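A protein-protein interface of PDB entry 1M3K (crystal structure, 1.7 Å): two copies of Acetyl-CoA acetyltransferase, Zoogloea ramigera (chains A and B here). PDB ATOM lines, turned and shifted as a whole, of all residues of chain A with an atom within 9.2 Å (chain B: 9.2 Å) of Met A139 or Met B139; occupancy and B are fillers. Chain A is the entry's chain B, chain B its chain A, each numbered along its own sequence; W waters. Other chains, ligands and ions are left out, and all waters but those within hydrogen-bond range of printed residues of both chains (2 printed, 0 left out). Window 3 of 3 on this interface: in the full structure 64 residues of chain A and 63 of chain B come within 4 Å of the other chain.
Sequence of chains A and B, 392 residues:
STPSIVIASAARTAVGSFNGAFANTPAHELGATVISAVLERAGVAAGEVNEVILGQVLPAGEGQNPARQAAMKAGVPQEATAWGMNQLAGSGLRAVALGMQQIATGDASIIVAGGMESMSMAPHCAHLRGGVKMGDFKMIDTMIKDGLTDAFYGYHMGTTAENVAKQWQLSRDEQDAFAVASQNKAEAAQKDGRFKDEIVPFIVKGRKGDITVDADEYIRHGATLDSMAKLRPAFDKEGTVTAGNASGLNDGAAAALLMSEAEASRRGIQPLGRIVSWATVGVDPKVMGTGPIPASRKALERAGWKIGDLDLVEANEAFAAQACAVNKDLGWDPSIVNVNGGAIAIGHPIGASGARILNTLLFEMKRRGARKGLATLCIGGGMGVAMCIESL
N of His A124 is in hydrogen-bond range of O of Ala B126. The backbone carbonyl oxygen (O) of Ala A126 sits at hydrogen-bond distance from the backbone NH (N) of His B124 (2.9 Å).
CG of Pro A123 touches CB of Cys B125, at 3.8 Å. Ala B126 touches Pro A123. CB of Pro A123 touches N of His B127, at 3.9 Å. His B124 touches His A124. Pro B123 touches Cys A125 (CG to CB, 3.8 Å). CA of Cys A125 touches O of His B124, 3.2 Å away. Cys B125 touches Cys A125 (CB to CB, 3.9 Å). CB of Pro B123 touches O of Ala A126 (3.2 Å). N of His A127 touches CB of Pro B123, at 3.8 Å. Met B139 touches Met A139 (CE to CE, 3.5 Å).
Pro A123 touches Ala B126, and with the chains exchanged Ala A126 touches Pro B123. Pro A123 touches His B127, and with the chains exchanged His A127 touches Pro B123. His A124 touches Cys B125, and with the chains exchanged Cys A125 touches His B124. Met B139 touches its own counterpart, Met A139. Of the 13 pairs that touch across the chains among the printed residues, 13 have their exchanged pair printed and touching as well.
The backbone carbonyl oxygen of Cys B125 sits at hydrogen-bond distance from the backbone NH of Ile B140, 2.7 Å away. OG1 of Thr B142 sits at hydrogen-bond distance from O of Pro B123, at 2.7 Å. The backbone NH (N) of Ile A140 sits at hydrogen-bond distance from the backbone carbonyl oxygen (O) of Cys A125, 2.7 Å away. OG1 of Thr A142 sits at hydrogen-bond distance from O of Pro A123 (2.6 Å).
Of the printed residues of chain B, Cys A125 touches Pro B123, His B124 and Cys B125. Of the printed residues of chain B, Ala A126 touches Pro B123 and His B124. Asp A136 touches none of the printed residues of chain B. Met A139 touches one residue of chain B. No residue of chain B comes within 4 Å of Ile A140. Met B139 touches just one residue of chain A: Met A139 (3.5 Å). The nearest printed residue of chain A that does not touch Ala B126 is Met A139 (5.0 Å).
Of the 15 printed residues of chain B, 6 touch a printed residue of chain A. Hydrophobic or aromatic side chains of chain B within 4 Å of the printed part of chain A: Pro B123 and Met B139. Of the 15 printed residues of chain A, 6 touch a printed residue of chain B. Hydrophobic or aromatic side chains of chain A within 4 Å of the printed part of chain B: Pro A123, His A124 and Met A139. Among the printed residues, 13 pairs touch across the chains. Among the printed residues, no Asp or Glu carboxylate lies within 4 Å of a Lys or Arg side-chain nitrogen of the other chain.
Water W1 bridges ND1 of His A124 and N of Leu B128. Water W2 bridges a ring nitrogen (ND1) of His B124 (2.9 Å) and the backbone NH of Leu A128 (2.9 Å).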
ATOM      1  N   PRO A 123     -28.423   3.623  13.589  1.00  0.00           N
ATOM      2  CA  PRO A 123     -26.956   3.565  13.667  1.00  0.00           C
ATOM      3  C   PRO A 123     -26.343   4.921  14.026  1.00  0.00           C
ATOM      4  O   PRO A 123     -27.052   5.925  14.024  1.00  0.00           O
ATOM      5  CB  PRO A 123     -26.547   3.194  12.258  1.00  0.00           C
ATOM      6  CG  PRO A 123     -27.499   3.825  11.420  1.00  0.00           C
ATOM      7  CD  PRO A 123     -28.868   3.743  12.209  1.00  0.00           C
ATOM      8  N   HIS A 124     -25.063   4.884  14.337  1.00  0.00           N
ATOM      9  CA  HIS A 124     -24.232   6.066  14.369  1.00  0.00           C
ATOM     10  C   HIS A 124     -23.626   6.388  12.990  1.00  0.00           C
ATOM     11  O   HIS A 124     -23.313   5.481  12.215  1.00  0.00           O
ATOM     12  CB  HIS A 124     -23.110   5.840  15.391  1.00  0.00           C
ATOM     13  CG  HIS A 124     -23.559   5.977  16.816  1.00  0.00           C
ATOM     14  ND1 HIS A 124     -24.393   5.063  17.428  1.00  0.00           N
ATOM     15  CD2 HIS A 124     -23.335   6.951  17.725  1.00  0.00           C
ATOM     16  CE1 HIS A 124     -24.621   5.444  18.679  1.00  0.00           C
ATOM     17  NE2 HIS A 124     -24.018   6.603  18.872  1.00  0.00           N
ATOM     18  N   CYS A 125     -23.393   7.656  12.673  1.00  0.00           N
ATOM     19  CA  CYS A 125     -22.875   7.927  11.350  1.00  0.00           C
ATOM     20  C   CYS A 125     -21.923   9.105  11.297  1.00  0.00           C
ATOM     21  O   CYS A 125     -21.762   9.854  12.262  1.00  0.00           O
ATOM     22  CB  CYS A 125     -24.014   8.181  10.349  1.00  0.00           C
ATOM     23  SG  CYS A 125     -24.899   9.728  10.619  1.00  0.00           S
ATOM     24  N   ALA A 126     -21.262   9.212  10.150  1.00  0.00           N
ATOM     25  CA  ALA A 126     -20.393  10.350   9.868  1.00  0.00           C
ATOM     26  C   ALA A 126     -20.151  10.415   8.392  1.00  0.00           C
ATOM     27  O   ALA A 126     -20.088   9.389   7.718  1.00  0.00           O
ATOM     28  CB  ALA A 126     -19.082  10.269  10.607  1.00  0.00           C
ATOM     29  N   HIS A 127     -20.094  11.636   7.866  1.00  0.00           N
ATOM     30  CA  HIS A 127     -19.777  11.879   6.491  1.00  0.00           C
ATOM     31  C   HIS A 127     -18.294  11.877   6.336  1.00  0.00           C
ATOM     32  O   HIS A 127     -17.592  12.755   6.843  1.00  0.00           O
ATOM     33  CB  HIS A 127     -20.339  13.240   6.032  1.00  0.00           C
ATOM     34  CG  HIS A 127     -19.977  13.620   4.623  1.00  0.00           C
ATOM     35  ND1 HIS A 127     -19.277  14.775   4.321  1.00  0.00           N
ATOM     36  CD2 HIS A 127     -20.283  13.041   3.431  1.00  0.00           C
ATOM     37  CE1 HIS A 127     -19.137  14.870   3.004  1.00  0.00           C
ATOM     38  NE2 HIS A 127     -19.757  13.840   2.439  1.00  0.00           N
ATOM     39  N   LEU A 128     -17.802  10.905   5.576  1.00  0.00           N
ATOM     40  CA  LEU A 128     -16.379  10.642   5.529  1.00  0.00           C
ATOM     41  C   LEU A 128     -15.772  10.697   4.132  1.00  0.00           C
ATOM     42  O   LEU A 128     -14.624  10.335   3.983  1.00  0.00           O
ATOM     43  CB  LEU A 128     -16.075   9.316   6.204  1.00  0.00           C
ATOM     44  CG  LEU A 128     -16.364   9.336   7.713  1.00  0.00           C
ATOM     45  CD1 LEU A 128     -16.320   7.979   8.270  1.00  0.00           C
ATOM     46  CD2 LEU A 128     -15.387  10.265   8.432  1.00  0.00           C
ATOM     47  N   ASP A 136     -10.433  16.117  15.309  1.00  0.00           N
ATOM     48  CA  ASP A 136     -11.456  15.171  15.752  1.00  0.00           C
ATOM     49  C   ASP A 136     -12.707  15.390  14.979  1.00  0.00           C
ATOM     50  O   ASP A 136     -12.910  16.458  14.362  1.00  0.00           O
ATOM     51  CB  ASP A 136     -11.717  15.324  17.275  1.00  0.00           C
ATOM     52  CG  ASP A 136     -10.470  15.092  18.120  1.00  0.00           C
ATOM     53  OD1 ASP A 136      -9.378  14.874  17.549  1.00  0.00           O
ATOM     54  OD2 ASP A 136     -10.470  15.127  19.373  1.00  0.00           O
ATOM     55  N   PHE A 137     -13.570  14.369  14.985  1.00  0.00           N
ATOM     56  CA  PHE A 137     -14.898  14.468  14.396  1.00  0.00           C
ATOM     57  C   PHE A 137     -15.907  13.598  15.171  1.00  0.00           C
ATOM     58  O   PHE A 137     -15.518  12.724  15.907  1.00  0.00           O
ATOM     59  CB  PHE A 137     -14.876  14.126  12.884  1.00  0.00           C
ATOM     60  CG  PHE A 137     -14.656  12.645  12.575  1.00  0.00           C
ATOM     61  CD1 PHE A 137     -13.375  12.117  12.474  1.00  0.00           C
ATOM     62  CD2 PHE A 137     -15.744  11.791  12.358  1.00  0.00           C
ATOM     63  CE1 PHE A 137     -13.164  10.774  12.183  1.00  0.00           C
ATOM     64  CE2 PHE A 137     -15.542  10.438  12.078  1.00  0.00           C
ATOM     65  CZ  PHE A 137     -14.246   9.927  11.981  1.00  0.00           C
ATOM     66  N   LYS A 138     -17.202  13.890  15.005  1.00  0.00           N
ATOM     67  CA  LYS A 138     -18.247  13.164  15.746  1.00  0.00           C
ATOM     68  C   LYS A 138     -18.798  11.997  14.906  1.00  0.00           C
ATOM     69  O   LYS A 138     -18.994  12.143  13.700  1.00  0.00           O
ATOM     70  CB  LYS A 138     -19.384  14.120  16.151  1.00  0.00           C
ATOM     71  CG  LYS A 138     -18.989  15.065  17.284  1.00  0.00           C
ATOM     72  CD  LYS A 138     -20.205  15.700  17.981  1.00  0.00           C
ATOM     73  CE  LYS A 138     -19.779  16.855  18.948  1.00  0.00           C
ATOM     74  NZ  LYS A 138     -20.850  17.908  19.139  1.00  0.00           N
ATOM     75  N   MET A 139     -18.983  10.850  15.575  1.00  0.00           N
ATOM     76  CA  MET A 139     -19.869   9.785  15.140  1.00  0.00           C
ATOM     77  C   MET A 139     -21.220  10.118  15.738  1.00  0.00           C
ATOM     78  O   MET A 139     -21.362  10.060  16.954  1.00  0.00           O
ATOM     79  CB  MET A 139     -19.351   8.423  15.624  1.00  0.00           C
ATOM     80  CG  MET A 139     -18.267   7.779  14.687  1.00  0.00           C
ATOM     81  SD  MET A 139     -18.916   7.329  13.064  1.00  0.00           S
ATOM     82  CE  MET A 139     -19.651   5.753  13.467  1.00  0.00           C
ATOM     83  N   ILE A 140     -22.176  10.449  14.864  1.00  0.00           N
ATOM     84  CA  ILE A 140     -23.446  11.064  15.256  1.00  0.00           C
ATOM     85  C   ILE A 140     -24.461   9.975  15.475  1.00  0.00           C
ATOM     86  O   ILE A 140     -24.633   9.137  14.601  1.00  0.00           O
ATOM     87  CB  ILE A 140     -23.864  12.001  14.132  1.00  0.00           C
ATOM     88  CG1 ILE A 140     -22.814  13.093  13.969  1.00  0.00           C
ATOM     89  CG2 ILE A 140     -25.264  12.531  14.345  1.00  0.00           C
ATOM     90  CD1 ILE A 140     -22.926  14.212  14.922  1.00  0.00           C
ATOM     91  N   ASP A 141     -25.193  10.032  16.595  1.00  0.00           N
ATOM     92  CA  ASP A 141     -26.311   9.108  16.825  1.00  0.00           C
ATOM     93  C   ASP A 141     -27.504   9.544  15.942  1.00  0.00           C
ATOM     94  O   ASP A 141     -28.101  10.586  16.143  1.00  0.00           O
ATOM     95  CB  ASP A 141     -26.607   9.102  18.333  1.00  0.00           C
ATOM     96  CG  ASP A 141     -27.626   8.070  18.730  1.00  0.00           C
ATOM     97  OD1 ASP A 141     -28.436   7.741  17.820  1.00  0.00           O
ATOM     98  OD2 ASP A 141     -27.625   7.550  19.872  1.00  0.00           O
ATOM     99  N   THR A 142     -27.834   8.789  14.893  1.00  0.00           N
ATOM    100  CA  THR A 142     -28.875   9.231  13.990  1.00  0.00           C
ATOM    101  C   THR A 142     -30.237   9.311  14.664  1.00  0.00           C
ATOM    102  O   THR A 142     -31.093  10.072  14.210  1.00  0.00           O
ATOM    103  CB  THR A 142     -29.086   8.295  12.756  1.00  0.00           C
ATOM    104  OG1 THR A 142     -29.331   6.923  13.174  1.00  0.00           O
ATOM    105  CG2 THR A 142     -27.882   8.346  11.848  1.00  0.00           C
ATOM    106  N   ILE A 144     -30.838  10.557  17.602  1.00  0.00           N
ATOM    107  CA  ILE A 144     -30.901  11.893  18.266  1.00  0.00           C
ATOM    108  C   ILE A 144     -30.930  13.006  17.221  1.00  0.00           C
ATOM    109  O   ILE A 144     -31.748  13.914  17.301  1.00  0.00           O
ATOM    110  CB  ILE A 144     -29.750  12.109  19.213  1.00  0.00           C
ATOM    111  CG1 ILE A 144     -29.827  11.107  20.394  1.00  0.00           C
ATOM    112  CG2 ILE A 144     -29.765  13.517  19.718  1.00  0.00           C
ATOM    113  CD1 ILE A 144     -28.583  10.955  21.229  1.00  0.00           C
ATOM    114  N   LYS A 145     -30.062  12.890  16.223  1.00  0.00           N
ATOM    115  CA  LYS A 145     -29.900  13.930  15.213  1.00  0.00           C
ATOM    116  C   LYS A 145     -31.093  14.013  14.288  1.00  0.00           C
ATOM    117  O   LYS A 145     -31.670  15.077  14.105  1.00  0.00           O
ATOM    118  CB  LYS A 145     -28.636  13.678  14.411  1.00  0.00           C
ATOM    119  CG  LYS A 145     -28.468  14.606  13.201  1.00  0.00           C
ATOM    120  CD  LYS A 145     -28.197  16.020  13.676  1.00  0.00           C
ATOM    121  CE  LYS A 145     -27.704  16.940  12.556  1.00  0.00           C
ATOM    122  NZ  LYS A 145     -27.272  18.307  13.029  1.00  0.00           N
ATOM    123  N   PRO B 123     -23.687   9.664   4.621  1.00  0.00           N
ATOM    124  CA  PRO B 123     -22.643   9.230   5.524  1.00  0.00           C
ATOM    125  C   PRO B 123     -22.429   7.722   5.487  1.00  0.00           C
ATOM    126  O   PRO B 123     -23.176   6.965   4.897  1.00  0.00           O
ATOM    127  CB  PRO B 123     -23.210   9.651   6.870  1.00  0.00           C
ATOM    128  CG  PRO B 123     -24.606   9.364   6.735  1.00  0.00           C
ATOM    129  CD  PRO B 123     -24.947   9.892   5.373  1.00  0.00           C
ATOM    130  N   HIS B 124     -21.415   7.321   6.169  1.00  0.00           N
ATOM    131  CA  HIS B 124     -21.212   5.917   6.485  1.00  0.00           C
ATOM    132  C   HIS B 124     -21.748   5.632   7.880  1.00  0.00           C
ATOM    133  O   HIS B 124     -21.667   6.497   8.753  1.00  0.00           O
ATOM    134  CB  HIS B 124     -19.732   5.595   6.463  1.00  0.00           C
ATOM    135  CG  HIS B 124     -19.129   5.500   5.090  1.00  0.00           C
ATOM    136  ND1 HIS B 124     -18.923   6.599   4.289  1.00  0.00           N
ATOM    137  CD2 HIS B 124     -18.575   4.449   4.437  1.00  0.00           C
ATOM    138  CE1 HIS B 124     -18.337   6.222   3.167  1.00  0.00           C
ATOM    139  NE2 HIS B 124     -18.134   4.918   3.221  1.00  0.00           N
ATOM    140  N   CYS B 125     -22.204   4.420   8.136  1.00  0.00           N
ATOM    141  CA  CYS B 125     -22.831   4.141   9.444  1.00  0.00           C
ATOM    142  C   CYS B 125     -22.560   2.749   9.944  1.00  0.00           C
ATOM    143  O   CYS B 125     -22.102   1.885   9.198  1.00  0.00           O
ATOM    144  CB  CYS B 125     -24.357   4.381   9.342  1.00  0.00           C
ATOM    145  SG  CYS B 125     -25.212   3.102   8.397  1.00  0.00           S
ATOM    146  N   ALA B 126     -22.828   2.544  11.243  1.00  0.00           N
ATOM    147  CA  ALA B 126     -22.789   1.216  11.870  1.00  0.00           C
ATOM    148  C   ALA B 126     -23.662   1.261  13.111  1.00  0.00           C
ATOM    149  O   ALA B 126     -23.747   2.320  13.793  1.00  0.00           O
ATOM    150  CB  ALA B 126     -21.454   0.915  12.238  1.00  0.00           C
ATOM    151  N   HIS B 127     -24.359   0.151  13.368  1.00  0.00           N
ATOM    152  CA  HIS B 127     -25.181   0.004  14.563  1.00  0.00           C
ATOM    153  C   HIS B 127     -24.271  -0.450  15.699  1.00  0.00           C
ATOM    154  O   HIS B 127     -23.762  -1.564  15.700  1.00  0.00           O
ATOM    155  CB  HIS B 127     -26.341  -0.980  14.320  1.00  0.00           C
ATOM    156  CG  HIS B 127     -27.083  -1.343  15.565  1.00  0.00           C
ATOM    157  ND1 HIS B 127     -26.914  -2.560  16.202  1.00  0.00           N
ATOM    158  CD2 HIS B 127     -27.911  -0.615  16.356  1.00  0.00           C
ATOM    159  CE1 HIS B 127     -27.649  -2.572  17.301  1.00  0.00           C
ATOM    160  NE2 HIS B 127     -28.262  -1.413  17.414  1.00  0.00           N
ATOM    161  N   LEU B 128     -24.050   0.426  16.677  1.00  0.00           N
ATOM    162  CA  LEU B 128     -23.035   0.257  17.700  1.00  0.00           C
ATOM    163  C   LEU B 128     -23.573   0.195  19.134  1.00  0.00           C
ATOM    164  O   LEU B 128     -22.801   0.108  20.074  1.00  0.00           O
ATOM    165  CB  LEU B 128     -22.024   1.399  17.586  1.00  0.00           C
ATOM    166  CG  LEU B 128     -21.140   1.268  16.347  1.00  0.00           C
ATOM    167  CD1 LEU B 128     -20.413   2.537  16.133  1.00  0.00           C
ATOM    168  CD2 LEU B 128     -20.203   0.140  16.478  1.00  0.00           C
ATOM    169  N   ASP B 136     -12.925  -6.337  14.419  1.00  0.00           N
ATOM    170  CA  ASP B 136     -13.278  -5.357  13.404  1.00  0.00           C
ATOM    171  C   ASP B 136     -14.777  -5.420  13.062  1.00  0.00           C
ATOM    172  O   ASP B 136     -15.408  -6.454  13.145  1.00  0.00           O
ATOM    173  CB  ASP B 136     -12.468  -5.561  12.102  1.00  0.00           C
ATOM    174  CG  ASP B 136     -11.096  -6.182  12.328  1.00  0.00           C
ATOM    175  OD1 ASP B 136     -10.379  -5.792  13.280  1.00  0.00           O
ATOM    176  OD2 ASP B 136     -10.641  -7.071  11.577  1.00  0.00           O
ATOM    177  N   PHE B 137     -15.322  -4.299  12.627  1.00  0.00           N
ATOM    178  CA  PHE B 137     -16.700  -4.255  12.119  1.00  0.00           C
ATOM    179  C   PHE B 137     -16.740  -3.300  10.917  1.00  0.00           C
ATOM    180  O   PHE B 137     -15.776  -2.556  10.667  1.00  0.00           O
ATOM    181  CB  PHE B 137     -17.689  -3.829  13.227  1.00  0.00           C
ATOM    182  CG  PHE B 137     -17.438  -2.473  13.746  1.00  0.00           C
ATOM    183  CD1 PHE B 137     -18.038  -1.347  13.137  1.00  0.00           C
ATOM    184  CD2 PHE B 137     -16.569  -2.277  14.781  1.00  0.00           C
ATOM    185  CE1 PHE B 137     -17.786  -0.084  13.606  1.00  0.00           C
ATOM    186  CE2 PHE B 137     -16.306  -0.987  15.263  1.00  0.00           C
ATOM    187  CZ  PHE B 137     -16.910   0.102  14.682  1.00  0.00           C
ATOM    188  N   LYS B 138     -17.824  -3.341  10.176  1.00  0.00           N
ATOM    189  CA  LYS B 138     -17.940  -2.532   8.942  1.00  0.00           C
ATOM    190  C   LYS B 138     -18.657  -1.218   9.168  1.00  0.00           C
ATOM    191  O   LYS B 138     -19.761  -1.148   9.769  1.00  0.00           O
ATOM    192  CB  LYS B 138     -18.718  -3.266   7.850  1.00  0.00           C
ATOM    193  CG  LYS B 138     -18.063  -4.467   7.181  1.00  0.00           C
ATOM    194  CD  LYS B 138     -19.025  -4.949   6.048  1.00  0.00           C
ATOM    195  CE  LYS B 138     -18.342  -5.086   4.689  1.00  0.00           C
ATOM    196  NZ  LYS B 138     -19.184  -4.525   3.574  1.00  0.00           N
ATOM    197  N   MET B 139     -18.063  -0.175   8.603  1.00  0.00           N
ATOM    198  CA  MET B 139     -18.745   1.056   8.429  1.00  0.00           C
ATOM    199  C   MET B 139     -19.355   0.981   7.032  1.00  0.00           C
ATOM    200  O   MET B 139     -18.608   0.845   6.036  1.00  0.00           O
ATOM    201  CB  MET B 139     -17.764   2.200   8.546  1.00  0.00           C
ATOM    202  CG  MET B 139     -17.369   2.459  10.006  1.00  0.00           C
ATOM    203  SD  MET B 139     -18.679   3.325  10.909  1.00  0.00           S
ATOM    204  CE  MET B 139     -18.500   5.039  10.255  1.00  0.00           C
ATOM    205  N   ILE B 140     -20.679   1.100   6.992  1.00  0.00           N
ATOM    206  CA  ILE B 140     -21.468   0.901   5.791  1.00  0.00           C
ATOM    207  C   ILE B 140     -21.692   2.229   5.080  1.00  0.00           C
ATOM    208  O   ILE B 140     -22.122   3.189   5.672  1.00  0.00           O
ATOM    209  CB  ILE B 140     -22.820   0.271   6.189  1.00  0.00           C
ATOM    210  CG1 ILE B 140     -22.635  -1.097   6.826  1.00  0.00           C
ATOM    211  CG2 ILE B 140     -23.745   0.147   4.989  1.00  0.00           C
ATOM    212  CD1 ILE B 140     -21.929  -2.017   5.926  1.00  0.00           C
ATOM    213  N   ASP B 141     -21.518   2.231   3.769  1.00  0.00           N
ATOM    214  CA  ASP B 141     -21.882   3.389   2.951  1.00  0.00           C
ATOM    215  C   ASP B 141     -23.394   3.459   2.749  1.00  0.00           C
ATOM    216  O   ASP B 141     -23.972   2.619   2.053  1.00  0.00           O
ATOM    217  CB  ASP B 141     -21.146   3.267   1.617  1.00  0.00           C
ATOM    218  CG  ASP B 141     -21.205   4.528   0.808  1.00  0.00           C
ATOM    219  OD1 ASP B 141     -22.155   5.267   1.028  1.00  0.00           O
ATOM    220  OD2 ASP B 141     -20.346   4.889  -0.049  1.00  0.00           O
ATOM    221  N   THR B 142     -24.056   4.399   3.404  1.00  0.00           N
ATOM    222  CA  THR B 142     -25.489   4.452   3.306  1.00  0.00           C
ATOM    223  C   THR B 142     -25.968   4.717   1.885  1.00  0.00           C
ATOM    224  O   THR B 142     -27.073   4.333   1.578  1.00  0.00           O
ATOM    225  CB  THR B 142     -26.141   5.481   4.206  1.00  0.00           C
ATOM    226  OG1 THR B 142     -25.680   6.805   3.882  1.00  0.00           O
ATOM    227  CG2 THR B 142     -25.861   5.217   5.706  1.00  0.00           C
ATOM    228  N   ILE B 144     -24.774   3.371  -0.903  1.00  0.00           N
ATOM    229  CA  ILE B 144     -24.787   2.047  -1.554  1.00  0.00           C
ATOM    230  C   ILE B 144     -25.885   1.151  -0.900  1.00  0.00           C
ATOM    231  O   ILE B 144     -26.689   0.530  -1.591  1.00  0.00           O
ATOM    232  CB  ILE B 144     -23.460   1.391  -1.512  1.00  0.00           C
ATOM    233  CG1 ILE B 144     -22.433   2.221  -2.262  1.00  0.00           C
ATOM    234  CG2 ILE B 144     -23.548  -0.014  -2.136  1.00  0.00           C
ATOM    235  CD1 ILE B 144     -21.044   1.797  -2.008  1.00  0.00           C
ATOM    236  N   LYS B 145     -25.916   1.096   0.425  1.00  0.00           N
ATOM    237  CA  LYS B 145     -26.851   0.182   1.153  1.00  0.00           C
ATOM    238  C   LYS B 145     -28.317   0.567   1.005  1.00  0.00           C
ATOM    239  O   LYS B 145     -29.179  -0.240   0.676  1.00  0.00           O
ATOM    240  CB  LYS B 145     -26.497   0.135   2.640  1.00  0.00           C
ATOM    241  CG  LYS B 145     -27.407  -0.745   3.538  1.00  0.00           C
ATOM    242  CD  LYS B 145     -27.248  -2.167   3.144  1.00  0.00           C
ATOM    243  CE  LYS B 145     -27.762  -3.104   4.249  1.00  0.00           C
ATOM    244  NZ  LYS B 145     -27.691  -4.554   3.958  1.00  0.00           N
HETATM  245  O   HOH W   1     -25.915   2.704  16.884  1.00  0.00           O
HETATM  246  O   HOH W   2     -19.599   9.374   3.886  1.00  0.00           O
